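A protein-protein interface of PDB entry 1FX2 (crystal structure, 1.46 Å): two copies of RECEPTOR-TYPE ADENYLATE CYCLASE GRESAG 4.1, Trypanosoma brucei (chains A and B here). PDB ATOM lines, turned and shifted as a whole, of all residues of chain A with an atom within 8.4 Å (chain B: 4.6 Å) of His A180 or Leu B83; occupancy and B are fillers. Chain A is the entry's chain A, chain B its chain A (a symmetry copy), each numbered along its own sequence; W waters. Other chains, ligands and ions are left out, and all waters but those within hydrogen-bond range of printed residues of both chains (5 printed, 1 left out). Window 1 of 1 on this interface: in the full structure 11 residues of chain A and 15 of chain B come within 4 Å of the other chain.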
ATOM      1  N   ILE A 138      26.000  14.121   7.437  1.00  0.00           N
ATOM      2  CA  ILE A 138      25.510  14.838   6.269  1.00  0.00           C
ATOM      3  C   ILE A 138      25.445  16.329   6.572  1.00  0.00           C
ATOM      4  O   ILE A 138      25.011  16.705   7.687  1.00  0.00           O
ATOM      5  CB  ILE A 138      24.051  14.417   5.890  1.00  0.00           C
ATOM      6  CG1 ILE A 138      23.985  12.901   5.644  1.00  0.00           C
ATOM      7  CG2 ILE A 138      23.609  15.167   4.582  1.00  0.00           C
ATOM      8  CD1 ILE A 138      22.559  12.431   5.430  1.00  0.00           C
ATOM      9  N   HIS A 139      26.028  17.143   5.675  1.00  0.00           N
ATOM     10  CA  HIS A 139      25.901  18.611   5.898  1.00  0.00           C
ATOM     11  C   HIS A 139      25.725  19.203   4.511  1.00  0.00           C
ATOM     12  O   HIS A 139      26.153  18.657   3.501  1.00  0.00           O
ATOM     13  CB  HIS A 139      27.209  19.146   6.554  1.00  0.00           C
ATOM     14  CG  HIS A 139      27.275  20.633   6.649  1.00  0.00           C
ATOM     15  ND1 HIS A 139      26.303  21.419   7.259  1.00  0.00           N
ATOM     16  CD2 HIS A 139      28.220  21.471   6.153  1.00  0.00           C
ATOM     17  CE1 HIS A 139      26.669  22.687   7.131  1.00  0.00           C
ATOM     18  NE2 HIS A 139      27.816  22.753   6.483  1.00  0.00           N
ATOM     19  N   THR A 140      25.139  20.406   4.463  1.00  0.00           N
ATOM     20  CA  THR A 140      24.886  21.106   3.178  1.00  0.00           C
ATOM     21  C   THR A 140      25.424  22.503   3.311  1.00  0.00           C
ATOM     22  O   THR A 140      25.179  23.144   4.333  1.00  0.00           O
ATOM     23  CB  THR A 140      23.397  21.223   2.909  1.00  0.00           C
ATOM     24  OG1 THR A 140      22.860  19.893   2.789  1.00  0.00           O
ATOM     25  CG2 THR A 140      23.178  22.021   1.594  1.00  0.00           C
ATOM     26  N   MET A 163      32.921  20.499   8.072  1.00  0.00           N
ATOM     27  CA  MET A 163      31.812  20.253   9.014  1.00  0.00           C
ATOM     28  C   MET A 163      31.155  18.912   8.761  1.00  0.00           C
ATOM     29  O   MET A 163      30.748  18.270   9.731  1.00  0.00           O
ATOM     30  CB  MET A 163      30.672  21.411   9.162  1.00  0.00           C
ATOM     31  CG  MET A 163      29.707  21.515  10.767  1.00  0.00           C
ATOM     32  SD  MET A 163      28.701  22.881  10.053  1.00  0.00           S
ATOM     33  CE  MET A 163      26.836  22.846  10.514  1.00  0.00           C
ATOM     34  N   THR A 167      31.000  16.116  11.632  1.00  0.00           N
ATOM     35  CA  THR A 167      29.681  15.642  12.042  1.00  0.00           C
ATOM     36  C   THR A 167      29.632  14.128  11.996  1.00  0.00           C
ATOM     37  O   THR A 167      29.175  13.465  12.915  1.00  0.00           O
ATOM     38  CB  THR A 167      28.603  16.195  11.101  1.00  0.00           C
ATOM     39  OG1 THR A 167      28.514  17.637  11.343  1.00  0.00           O
ATOM     40  CG2 THR A 167      27.218  15.612  11.372  1.00  0.00           C
ATOM     41  N   LEU A 177      23.749  11.249  11.232  1.00  0.00           N
ATOM     42  CA  LEU A 177      23.542  12.611  11.736  1.00  0.00           C
ATOM     43  C   LEU A 177      23.532  13.597  10.597  1.00  0.00           C
ATOM     44  O   LEU A 177      24.294  13.460   9.612  1.00  0.00           O
ATOM     45  CB  LEU A 177      24.733  13.004  12.632  1.00  0.00           C
ATOM     46  CG  LEU A 177      24.842  12.112  13.898  1.00  0.00           C
ATOM     47  CD1 LEU A 177      26.075  12.624  14.756  1.00  0.00           C
ATOM     48  CD2 LEU A 177      23.573  12.070  14.762  1.00  0.00           C
ATOM     49  N   MET A 178      22.658  14.579  10.712  1.00  0.00           N
ATOM     50  CA  MET A 178      22.574  15.662   9.739  1.00  0.00           C
ATOM     51  C   MET A 178      22.702  16.968  10.515  1.00  0.00           C
ATOM     52  O   MET A 178      22.107  17.118  11.608  1.00  0.00           O
ATOM     53  CB  MET A 178      21.198  15.672   9.030  1.00  0.00           C
ATOM     54  CG  MET A 178      20.706  14.385   8.290  1.00  0.00           C
ATOM     55  SD  MET A 178      18.891  14.542   7.901  1.00  0.00           S
ATOM     56  CE  MET A 178      18.953  16.042   7.783  1.00  0.00           C
ATOM     57  N   THR A 179      23.402  17.938   9.961  1.00  0.00           N
ATOM     58  CA  THR A 179      23.405  19.244  10.638  1.00  0.00           C
ATOM     59  C   THR A 179      22.055  19.907  10.400  1.00  0.00           C
ATOM     60  O   THR A 179      21.301  19.550   9.481  1.00  0.00           O
ATOM     61  CB  THR A 179      24.491  20.180  10.006  1.00  0.00           C
ATOM     62  OG1 THR A 179      24.180  20.268   8.586  1.00  0.00           O
ATOM     63  CG2 THR A 179      25.895  19.536  10.177  1.00  0.00           C
ATOM     64  N   HIS A 180      21.776  20.927  11.175  1.00  0.00           N
ATOM     65  CA  HIS A 180      20.556  21.672  10.904  1.00  0.00           C
ATOM     66  C   HIS A 180      20.587  22.264   9.519  1.00  0.00           C
ATOM     67  O   HIS A 180      19.549  22.389   8.906  1.00  0.00           O
ATOM     68  CB  HIS A 180      20.399  22.774  11.978  1.00  0.00           C
ATOM     69  CG  HIS A 180      19.117  23.543  11.850  1.00  0.00           C
ATOM     70  ND1 HIS A 180      19.007  24.782  11.267  1.00  0.00           N
ATOM     71  CD2 HIS A 180      17.867  23.172  12.217  1.00  0.00           C
ATOM     72  CE1 HIS A 180      17.726  25.144  11.280  1.00  0.00           C
ATOM     73  NE2 HIS A 180      17.028  24.185  11.854  1.00  0.00           N
ATOM     74  N   ALA A 181      21.738  22.690   9.010  1.00  0.00           N
ATOM     75  CA  ALA A 181      21.816  23.212   7.679  1.00  0.00           C
ATOM     76  C   ALA A 181      21.319  22.286   6.645  1.00  0.00           C
ATOM     77  O   ALA A 181      20.532  22.624   5.777  1.00  0.00           O
ATOM     78  CB  ALA A 181      23.258  23.698   7.358  1.00  0.00           C
ATOM     79  N   ALA A 182      21.714  20.976   6.789  1.00  0.00           N
ATOM     80  CA  ALA A 182      21.214  20.026   5.827  1.00  0.00           C
ATOM     81  C   ALA A 182      19.707  19.827   6.007  1.00  0.00           C
ATOM     82  O   ALA A 182      18.980  19.690   5.020  1.00  0.00           O
ATOM     83  CB  ALA A 182      21.934  18.673   6.033  1.00  0.00           C
ATOM     84  N   TYR A 183      19.233  19.710   7.236  1.00  0.00           N
ATOM     85  CA  TYR A 183      17.804  19.471   7.499  1.00  0.00           C
ATOM     86  C   TYR A 183      16.981  20.592   6.904  1.00  0.00           C
ATOM     87  O   TYR A 183      16.021  20.296   6.172  1.00  0.00           O
ATOM     88  CB  TYR A 183      17.573  19.377   9.000  1.00  0.00           C
ATOM     89  CG  TYR A 183      16.132  19.056   9.354  1.00  0.00           C
ATOM     90  CD1 TYR A 183      15.620  17.810   8.991  1.00  0.00           C
ATOM     91  CD2 TYR A 183      15.318  19.929  10.050  1.00  0.00           C
ATOM     92  CE1 TYR A 183      14.302  17.464   9.299  1.00  0.00           C
ATOM     93  CE2 TYR A 183      13.992  19.558  10.386  1.00  0.00           C
ATOM     94  CZ  TYR A 183      13.511  18.336   9.992  1.00  0.00           C
ATOM     95  OH  TYR A 183      12.169  17.992  10.296  1.00  0.00           O
ATOM     96  N   MET A 184      17.386  21.871   7.065  1.00  0.00           N
ATOM     97  CA  MET A 184      16.561  22.928   6.537  1.00  0.00           C
ATOM     98  C   MET A 184      16.831  23.189   5.052  1.00  0.00           C
ATOM     99  O   MET A 184      16.087  24.013   4.455  1.00  0.00           O
ATOM    100  CB  MET A 184      16.446  24.156   7.594  1.00  0.00           C
ATOM    101  CG  MET A 184      15.161  23.977   8.755  1.00  0.00           C
ATOM    102  SD  MET A 184      13.870  23.785   8.255  1.00  0.00           S
ATOM    103  CE  MET A 184      13.680  25.378   7.437  1.00  0.00           C
ATOM    104  N   SER A 185      17.791  22.490   4.410  1.00  0.00           N
ATOM    105  CA  SER A 185      18.011  22.555   2.950  1.00  0.00           C
ATOM    106  C   SER A 185      16.949  21.750   2.233  1.00  0.00           C
ATOM    107  O   SER A 185      16.842  21.770   0.994  1.00  0.00           O
ATOM    108  CB  SER A 185      19.410  22.127   2.575  1.00  0.00           C
ATOM    109  OG  SER A 185      20.306  23.054   3.125  1.00  0.00           O
ATOM    110  N   LEU A 186      16.333  20.820   2.959  1.00  0.00           N
ATOM    111  CA  LEU A 186      15.290  20.005   2.382  1.00  0.00           C
ATOM    112  C   LEU A 186      14.041  20.860   2.281  1.00  0.00           C
ATOM    113  O   LEU A 186      13.813  21.757   3.118  1.00  0.00           O
ATOM    114  CB  LEU A 186      14.923  18.881   3.376  1.00  0.00           C
ATOM    115  CG  LEU A 186      16.089  17.934   3.655  1.00  0.00           C
ATOM    116  CD1 LEU A 186      15.708  16.973   4.817  1.00  0.00           C
ATOM    117  CD2 LEU A 186      16.401  17.153   2.432  1.00  0.00           C
ATOM    118  N   ARG A 191      10.779  17.165   4.213  1.00  0.00           N
ATOM    119  CA  ARG A 191      10.851  16.883   5.627  1.00  0.00           C
ATOM    120  C   ARG A 191       9.708  16.032   6.142  1.00  0.00           C
ATOM    121  O   ARG A 191       9.820  15.381   7.190  1.00  0.00           O
ATOM    122  CB  ARG A 191      10.970  18.153   6.473  1.00  0.00           C
ATOM    123  CG  ARG A 191      12.361  18.751   6.223  1.00  0.00           C
ATOM    124  CD  ARG A 191      12.641  19.920   7.184  1.00  0.00           C
ATOM    125  NE  ARG A 191      11.788  21.015   6.862  1.00  0.00           N
ATOM    126  CZ  ARG A 191      12.163  21.913   6.012  1.00  0.00           C
ATOM    127  NH1 ARG A 191      13.372  21.796   5.477  1.00  0.00           N
ATOM    128  NH2 ARG A 191      11.359  22.951   5.767  1.00  0.00           N
ATOM    129  N   ALA A 198      15.928  15.502  17.293  1.00  0.00           N
ATOM    130  CA  ALA A 198      16.907  16.515  17.640  1.00  0.00           C
ATOM    131  C   ALA A 198      17.852  16.054  18.715  1.00  0.00           C
ATOM    132  O   ALA A 198      17.427  15.530  19.738  1.00  0.00           O
ATOM    133  CB  ALA A 198      16.187  17.820  18.163  1.00  0.00           C
ATOM    134  N   LEU A 199      19.143  16.327  18.519  1.00  0.00           N
ATOM    135  CA  LEU A 199      20.106  15.974  19.506  1.00  0.00           C
ATOM    136  C   LEU A 199      20.701  17.264  20.136  1.00  0.00           C
ATOM    137  O   LEU A 199      21.644  17.141  20.903  1.00  0.00           O
ATOM    138  CB  LEU A 199      21.208  15.050  18.893  1.00  0.00           C
ATOM    139  CG  LEU A 199      20.733  13.677  18.317  1.00  0.00           C
ATOM    140  CD1 LEU A 199      21.914  12.846  17.807  1.00  0.00           C
ATOM    141  CD2 LEU A 199      19.977  12.814  19.265  1.00  0.00           C
ATOM    142  N   GLY A 200      20.147  18.439  19.873  1.00  0.00           N
ATOM    143  CA  GLY A 200      20.652  19.697  20.496  1.00  0.00           C
ATOM    144  C   GLY A 200      21.772  20.403  19.731  1.00  0.00           C
ATOM    145  O   GLY A 200      21.684  20.556  18.506  1.00  0.00           O
ATOM    146  N   ASP A 201      22.886  20.689  20.409  1.00  0.00           N
ATOM    147  CA  ASP A 201      24.113  21.264  19.769  1.00  0.00           C
ATOM    148  C   ASP A 201      25.333  20.595  20.326  1.00  0.00           C
ATOM    149  O   ASP A 201      25.428  20.346  21.526  1.00  0.00           O
ATOM    150  CB  ASP A 201      24.366  22.779  19.853  1.00  0.00           C
ATOM    151  CG  ASP A 201      23.263  23.581  20.481  1.00  0.00           C
ATOM    152  OD1 ASP A 201      22.187  23.025  20.798  1.00  0.00           O
ATOM    153  OD2 ASP A 201      23.501  24.818  20.656  1.00  0.00           O
ATOM    154  N   PRO A 210      29.084  25.740  18.189  1.00  0.00           N
ATOM    155  CA  PRO A 210      28.467  24.402  18.325  1.00  0.00           C
ATOM    156  C   PRO A 210      27.447  24.214  17.219  1.00  0.00           C
ATOM    157  O   PRO A 210      26.792  25.174  16.774  1.00  0.00           O
ATOM    158  CB  PRO A 210      27.748  24.443  19.663  1.00  0.00           C
ATOM    159  CG  PRO A 210      28.465  25.626  20.399  1.00  0.00           C
ATOM    160  CD  PRO A 210      28.878  26.583  19.385  1.00  0.00           C
ATOM    161  N   VAL A 211      27.325  22.945  16.826  1.00  0.00           N
ATOM    162  CA  VAL A 211      26.482  22.582  15.697  1.00  0.00           C
ATOM    163  C   VAL A 211      25.263  21.809  16.184  1.00  0.00           C
ATOM    164  O   VAL A 211      25.396  20.818  16.876  1.00  0.00           O
ATOM    165  CB  VAL A 211      27.298  21.693  14.712  1.00  0.00           C
ATOM    166  CG1 VAL A 211      26.408  21.222  13.535  1.00  0.00           C
ATOM    167  CG2 VAL A 211      28.450  22.548  14.141  1.00  0.00           C
ATOM    168  N   LYS A 212      24.075  22.253  15.745  1.00  0.00           N
ATOM    169  CA  LYS A 212      22.820  21.596  16.136  1.00  0.00           C
ATOM    170  C   LYS A 212      22.706  20.349  15.210  1.00  0.00           C
ATOM    171  O   LYS A 212      22.744  20.545  13.973  1.00  0.00           O
ATOM    172  CB  LYS A 212      21.651  22.552  15.895  1.00  0.00           C
ATOM    173  CG  LYS A 212      21.465  23.619  16.985  1.00  0.00           C
ATOM    174  CD  LYS A 212      22.153  24.955  16.649  1.00  0.00           C
ATOM    175  CE  LYS A 212      22.231  25.868  17.888  1.00  0.00           C
ATOM    176  NZ  LYS A 212      22.848  27.181  17.483  1.00  0.00           N
ATOM    177  N   MET A 213      22.625  19.175  15.826  1.00  0.00           N
ATOM    178  CA  MET A 213      22.592  17.886  15.152  1.00  0.00           C
ATOM    179  C   MET A 213      21.236  17.260  15.173  1.00  0.00           C
ATOM    180  O   MET A 213      20.488  17.394  16.163  1.00  0.00           O
ATOM    181  CB  MET A 213      23.516  16.883  15.837  1.00  0.00           C
ATOM    182  CG  MET A 213      24.902  17.196  15.817  1.00  0.00           C
ATOM    183  SD  MET A 213      25.414  17.216  14.107  1.00  0.00           S
ATOM    184  CE  MET A 213      27.103  17.739  14.526  1.00  0.00           C
ATOM    185  N   TYR A 214      20.889  16.570  14.082  1.00  0.00           N
ATOM    186  CA  TYR A 214      19.669  15.849  13.988  1.00  0.00           C
ATOM    187  C   TYR A 214      19.998  14.409  13.629  1.00  0.00           C
ATOM    188  O   TYR A 214      20.757  14.167  12.692  1.00  0.00           O
ATOM    189  CB  TYR A 214      18.772  16.478  12.907  1.00  0.00           C
ATOM    190  CG  TYR A 214      18.191  17.784  13.355  1.00  0.00           C
ATOM    191  CD1 TYR A 214      18.976  18.937  13.355  1.00  0.00           C
ATOM    192  CD2 TYR A 214      16.948  17.813  13.966  1.00  0.00           C
ATOM    193  CE1 TYR A 214      18.527  20.091  13.997  1.00  0.00           C
ATOM    194  CE2 TYR A 214      16.487  18.989  14.581  1.00  0.00           C
ATOM    195  CZ  TYR A 214      17.320  20.070  14.579  1.00  0.00           C
ATOM    196  OH  TYR A 214      16.832  21.229  15.204  1.00  0.00           O
ATOM    197  N   GLN B  79      16.023  27.186  22.877  1.00  0.00           N
ATOM    198  CA  GLN B  79      16.592  26.868  21.592  1.00  0.00           C
ATOM    199  C   GLN B  79      15.636  25.952  20.807  1.00  0.00           C
ATOM    200  O   GLN B  79      15.385  26.189  19.591  1.00  0.00           O
ATOM    201  CB  GLN B  79      17.948  26.267  21.825  1.00  0.00           C
ATOM    202  CG  GLN B  79      18.653  25.782  20.618  1.00  0.00           C
ATOM    203  CD  GLN B  79      20.150  25.693  20.952  1.00  0.00           C
ATOM    204  OE1 GLN B  79      20.885  26.660  20.780  1.00  0.00           O
ATOM    205  NE2 GLN B  79      20.553  24.585  21.523  1.00  0.00           N
ATOM    206  N   GLU B  80      15.080  24.916  21.452  1.00  0.00           N
ATOM    207  CA  GLU B  80      14.156  23.991  20.740  1.00  0.00           C
ATOM    208  C   GLU B  80      12.817  24.592  20.393  1.00  0.00           C
ATOM    209  O   GLU B  80      12.082  24.187  19.467  1.00  0.00           O
ATOM    210  CB  GLU B  80      13.947  22.672  21.547  1.00  0.00           C
ATOM    211  CG  GLU B  80      15.170  21.812  21.585  1.00  0.00           C
ATOM    212  CD  GLU B  80      15.759  21.476  20.231  1.00  0.00           C
ATOM    213  OE1 GLU B  80      14.968  21.243  19.273  1.00  0.00           O
ATOM    214  OE2 GLU B  80      17.010  21.409  20.080  1.00  0.00           O
ATOM    215  N   LEU B  81      12.484  25.625  21.108  1.00  0.00           N
ATOM    216  CA  LEU B  81      11.221  26.314  20.824  1.00  0.00           C
ATOM    217  C   LEU B  81      11.489  27.028  19.463  1.00  0.00           C
ATOM    218  O   LEU B  81      10.677  26.867  18.517  1.00  0.00           O
ATOM    219  CB  LEU B  81      10.938  27.341  21.924  1.00  0.00           C
ATOM    220  CG  LEU B  81       9.580  28.068  21.787  1.00  0.00           C
ATOM    221  CD1 LEU B  81       9.217  28.744  23.137  1.00  0.00           C
ATOM    222  CD2 LEU B  81       9.647  29.251  20.782  1.00  0.00           C
ATOM    223  N   GLN B  82      12.572  27.755  19.288  1.00  0.00           N
ATOM    224  CA  GLN B  82      12.788  28.439  18.028  1.00  0.00           C
ATOM    225  C   GLN B  82      12.885  27.466  16.868  1.00  0.00           C
ATOM    226  O   GLN B  82      12.299  27.713  15.798  1.00  0.00           O
ATOM    227  CB  GLN B  82      14.047  29.308  18.091  1.00  0.00           C
ATOM    228  CG  GLN B  82      13.982  30.456  19.191  1.00  0.00           C
ATOM    229  CD  GLN B  82      12.917  31.496  18.840  1.00  0.00           C
ATOM    230  OE1 GLN B  82      12.444  31.547  17.686  1.00  0.00           O
ATOM    231  NE2 GLN B  82      12.427  32.182  19.837  1.00  0.00           N
ATOM    232  N   LEU B  83      13.621  26.346  17.073  1.00  0.00           N
ATOM    233  CA  LEU B  83      13.783  25.350  16.022  1.00  0.00           C
ATOM    234  C   LEU B  83      12.471  24.610  15.691  1.00  0.00           C
ATOM    235  O   LEU B  83      12.127  24.535  14.503  1.00  0.00           O
ATOM    236  CB  LEU B  83      14.882  24.366  16.401  1.00  0.00           C
ATOM    237  CG  LEU B  83      16.250  25.058  16.511  1.00  0.00           C
ATOM    238  CD1 LEU B  83      17.206  24.111  17.301  1.00  0.00           C
ATOM    239  CD2 LEU B  83      16.848  25.297  15.113  1.00  0.00           C
ATOM    240  N   CYS B  84      11.697  24.117  16.642  1.00  0.00           N
ATOM    241  CA  CYS B  84      10.496  23.432  16.198  1.00  0.00           C
ATOM    242  C   CYS B  84       9.446  24.372  15.632  1.00  0.00           C
ATOM    243  O   CYS B  84       8.552  23.963  14.829  1.00  0.00           O
ATOM    244  CB  CYS B  84       9.901  22.536  17.244  1.00  0.00           C
ATOM    245  SG  CYS B  84       9.341  23.359  18.639  1.00  0.00           S
ATOM    246  N   PHE B  85       9.424  25.613  16.092  1.00  0.00           N
ATOM    247  CA  PHE B  85       8.493  26.514  15.418  1.00  0.00           C
ATOM    248  C   PHE B  85       8.920  26.737  13.976  1.00  0.00           C
ATOM    249  O   PHE B  85       8.056  26.804  13.049  1.00  0.00           O
ATOM    250  CB  PHE B  85       8.431  27.861  16.162  1.00  0.00           C
ATOM    251  CG  PHE B  85       7.433  27.877  17.282  1.00  0.00           C
ATOM    252  CD1 PHE B  85       7.502  26.976  18.325  1.00  0.00           C
ATOM    253  CD2 PHE B  85       6.403  28.852  17.280  1.00  0.00           C
ATOM    254  CE1 PHE B  85       6.579  27.027  19.406  1.00  0.00           C
ATOM    255  CE2 PHE B  85       5.477  28.882  18.342  1.00  0.00           C
ATOM    256  CZ  PHE B  85       5.591  27.957  19.415  1.00  0.00           C
ATOM    257  N   LEU B  86      10.219  26.821  13.689  1.00  0.00           N
ATOM    258  CA  LEU B  86      10.694  27.010  12.321  1.00  0.00           C
ATOM    259  C   LEU B  86      10.321  25.777  11.479  1.00  0.00           C
ATOM    260  O   LEU B  86       9.917  25.868  10.303  1.00  0.00           O
ATOM    261  CB  LEU B  86      12.227  27.181  12.349  1.00  0.00           C
ATOM    262  CG  LEU B  86      12.870  27.097  10.943  1.00  0.00           C
ATOM    263  CD1 LEU B  86      12.525  28.423  10.111  1.00  0.00           C
ATOM    264  CD2 LEU B  86      14.429  27.166  11.199  1.00  0.00           C
ATOM    265  N   HIS B  87      10.396  24.605  12.116  1.00  0.00           N
ATOM    266  CA  HIS B  87      10.132  23.353  11.377  1.00  0.00           C
ATOM    267  C   HIS B  87       8.674  23.028  11.191  1.00  0.00           C
ATOM    268  O   HIS B  87       8.304  22.352  10.223  1.00  0.00           O
ATOM    269  CB  HIS B  87      10.796  22.187  12.084  1.00  0.00           C
ATOM    270  CG  HIS B  87      12.277  22.354  12.239  1.00  0.00           C
ATOM    271  ND1 HIS B  87      12.996  21.720  13.244  1.00  0.00           N
ATOM    272  CD2 HIS B  87      13.152  23.165  11.594  1.00  0.00           C
ATOM    273  CE1 HIS B  87      14.252  22.148  13.191  1.00  0.00           C
ATOM    274  NE2 HIS B  87      14.387  23.007  12.202  1.00  0.00           N
ATOM    275  N   THR B 218      20.139  30.386  17.981  1.00  0.00           N
ATOM    276  CA  THR B 218      19.334  29.140  17.905  1.00  0.00           C
ATOM    277  C   THR B 218      19.342  28.707  16.429  1.00  0.00           C
ATOM    278  O   THR B 218      20.076  27.798  16.019  1.00  0.00           O
ATOM    279  CB  THR B 218      17.871  29.335  18.491  1.00  0.00           C
ATOM    280  OG1 THR B 218      17.124  30.314  17.758  1.00  0.00           O
ATOM    281  CG2 THR B 218      17.960  29.860  19.935  1.00  0.00           C
ATOM    282  N   VAL B 219      18.440  29.308  15.654  1.00  0.00           N
ATOM    283  CA  VAL B 219      18.418  29.087  14.189  1.00  0.00           C
ATOM    284  C   VAL B 219      19.683  29.744  13.642  1.00  0.00           C
ATOM    285  O   VAL B 219      19.954  30.962  13.690  1.00  0.00           O
ATOM    286  CB  VAL B 219      17.219  29.699  13.648  1.00  0.00           C
ATOM    287  CG1 VAL B 219      17.225  29.606  12.121  1.00  0.00           C
ATOM    288  CG2 VAL B 219      16.051  28.974  14.206  1.00  0.00           C
ATOM    289  N   PRO B 220      20.528  28.939  13.034  1.00  0.00           N
ATOM    290  CA  PRO B 220      21.768  29.524  12.526  1.00  0.00           C
ATOM    291  C   PRO B 220      21.601  30.643  11.415  1.00  0.00           C
ATOM    292  O   PRO B 220      20.766  30.493  10.557  1.00  0.00           O
ATOM    293  CB  PRO B 220      22.528  28.278  11.979  1.00  0.00           C
ATOM    294  CG  PRO B 220      21.781  27.080  12.596  1.00  0.00           C
ATOM    295  CD  PRO B 220      20.375  27.499  12.714  1.00  0.00           C
HETATM  296  O   HOH W   1      18.765  20.644  17.673  1.00  0.00           O
HETATM  297  O   HOH W   2       9.788  24.992   7.636  1.00  0.00           O
HETATM  298  O   HOH W   3       9.891  20.642   8.842  1.00  0.00           O
HETATM  299  O   HOH W   4      23.216  27.960  20.766  1.00  0.00           O
HETATM  300  O   HOH W   5      14.784  20.828  16.712  1.00  0.00           O
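Hydrophobic or aromatic side chains of chain A that line the printed part of chain B: His A180, Tyr A183, Met A184, Ala A198 and Tyr A214.
Of the 12 printed residues of chain B, 7 touch a printed residue of chain A.
Ile A138 touches none of the printed residues of chain B.
Of chain B, only Leu B83, Leu B86, His B87 and Pro B220 come within 4 Å of His A180.
Of the printed residues of chain B, Tyr A183 touches His B87.
Of the printed residues of chain B, Met A184 touches Leu B86 (3.99 Å) and His B87 (3.5 Å).
Pro A210 touches none of the printed residues of chain B.
Leu B83 touches just these residues of chain A: His A180 (3.4 Å) and Tyr A214 (3.6 Å).
The nearest residue of chain A that does not touch Leu B83 is Lys A212 (4.3 Å).
The nearest printed residue of chain A that does not touch Gln B79 is Gly A200 (4.7 Å).
Among the printed residues, merely in contact across the chains: His A180 with Leu B83, His A180 with Leu B86, His A180 with Pro B220, Tyr A183 with His B87, Met A184 with Leu B86, Met A184 with His B87, Ala A198 with Glu B80, Lys A212 with Gln B79, Tyr A214 with Leu B83 and Tyr A214 with His B87.
NE2 of His B87 is in hydrogen-bond range of NE2 of His A180, 2.9 Å away.
The side-chain carboxylate (OD2) of Asp A201 sits close to the side-chain amide nitrogen (NE2) of Gln B79 (3.1 Å).
The side-chain amino group (NZ) of Lys A212 sits at hydrogen-bond distance from the backbone carbonyl oxygen (O) of Thr B218, at 3.2 Å.
Water W5 lies within hydrogen-bond range of the side-chain hydroxyl of Tyr A214 (2.6 Å) and the side-chain carboxylate of Glu B80 (2.6 Å).
Water W4 lies within hydrogen-bond range of the side-chain amide oxygen (OE1) of Gln B79 (2.7 Å), the side-chain carboxylate (OD2) of Asp A201 (3.2 Å) and the side-chain amino group (NZ) of Lys A212 (3.4 Å).
Water W3 bridges the backbone carbonyl oxygen of His B87 and the guanidinium group of Arg A191.
Water W2 lies within hydrogen-bond range of the backbone carbonyl oxygen (O) of Leu B86 (2.8 Å) and the guanidinium group (NH2) of Arg A191 (3.2 Å).
Water W1 lies within hydrogen-bond range of O of Gly A200 (3.0 Å), OE2 of Glu B80 (3.1 Å) and OH of Tyr A214 (3.2 Å).
No position is printed for both chains.
Of the 13 pairs that touch across the chains among the printed residues, none has its exchanged pair printed and touching as well.
O of Tyr A214 is in hydrogen-bond range of N of Met A178, 2.8 Å away.
N of His A180 sits at hydrogen-bond distance from O of Lys A212, 3.0 Å away.
O of Tyr A183 lies within hydrogen-bond range of NH1 of Arg A191 (3.1 Å).
SD of Met A184 sits close to NH1 of Arg A191 (3.5 Å).
The backbone carbonyl oxygen (O) of Glu B80 sits at hydrogen-bond distance from the side-chain sulfur (SG) of Cys B84, 3.0 Å away.
The backbone carbonyl oxygen of Leu B83 sits close to a ring nitrogen (ND1) of His B87.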
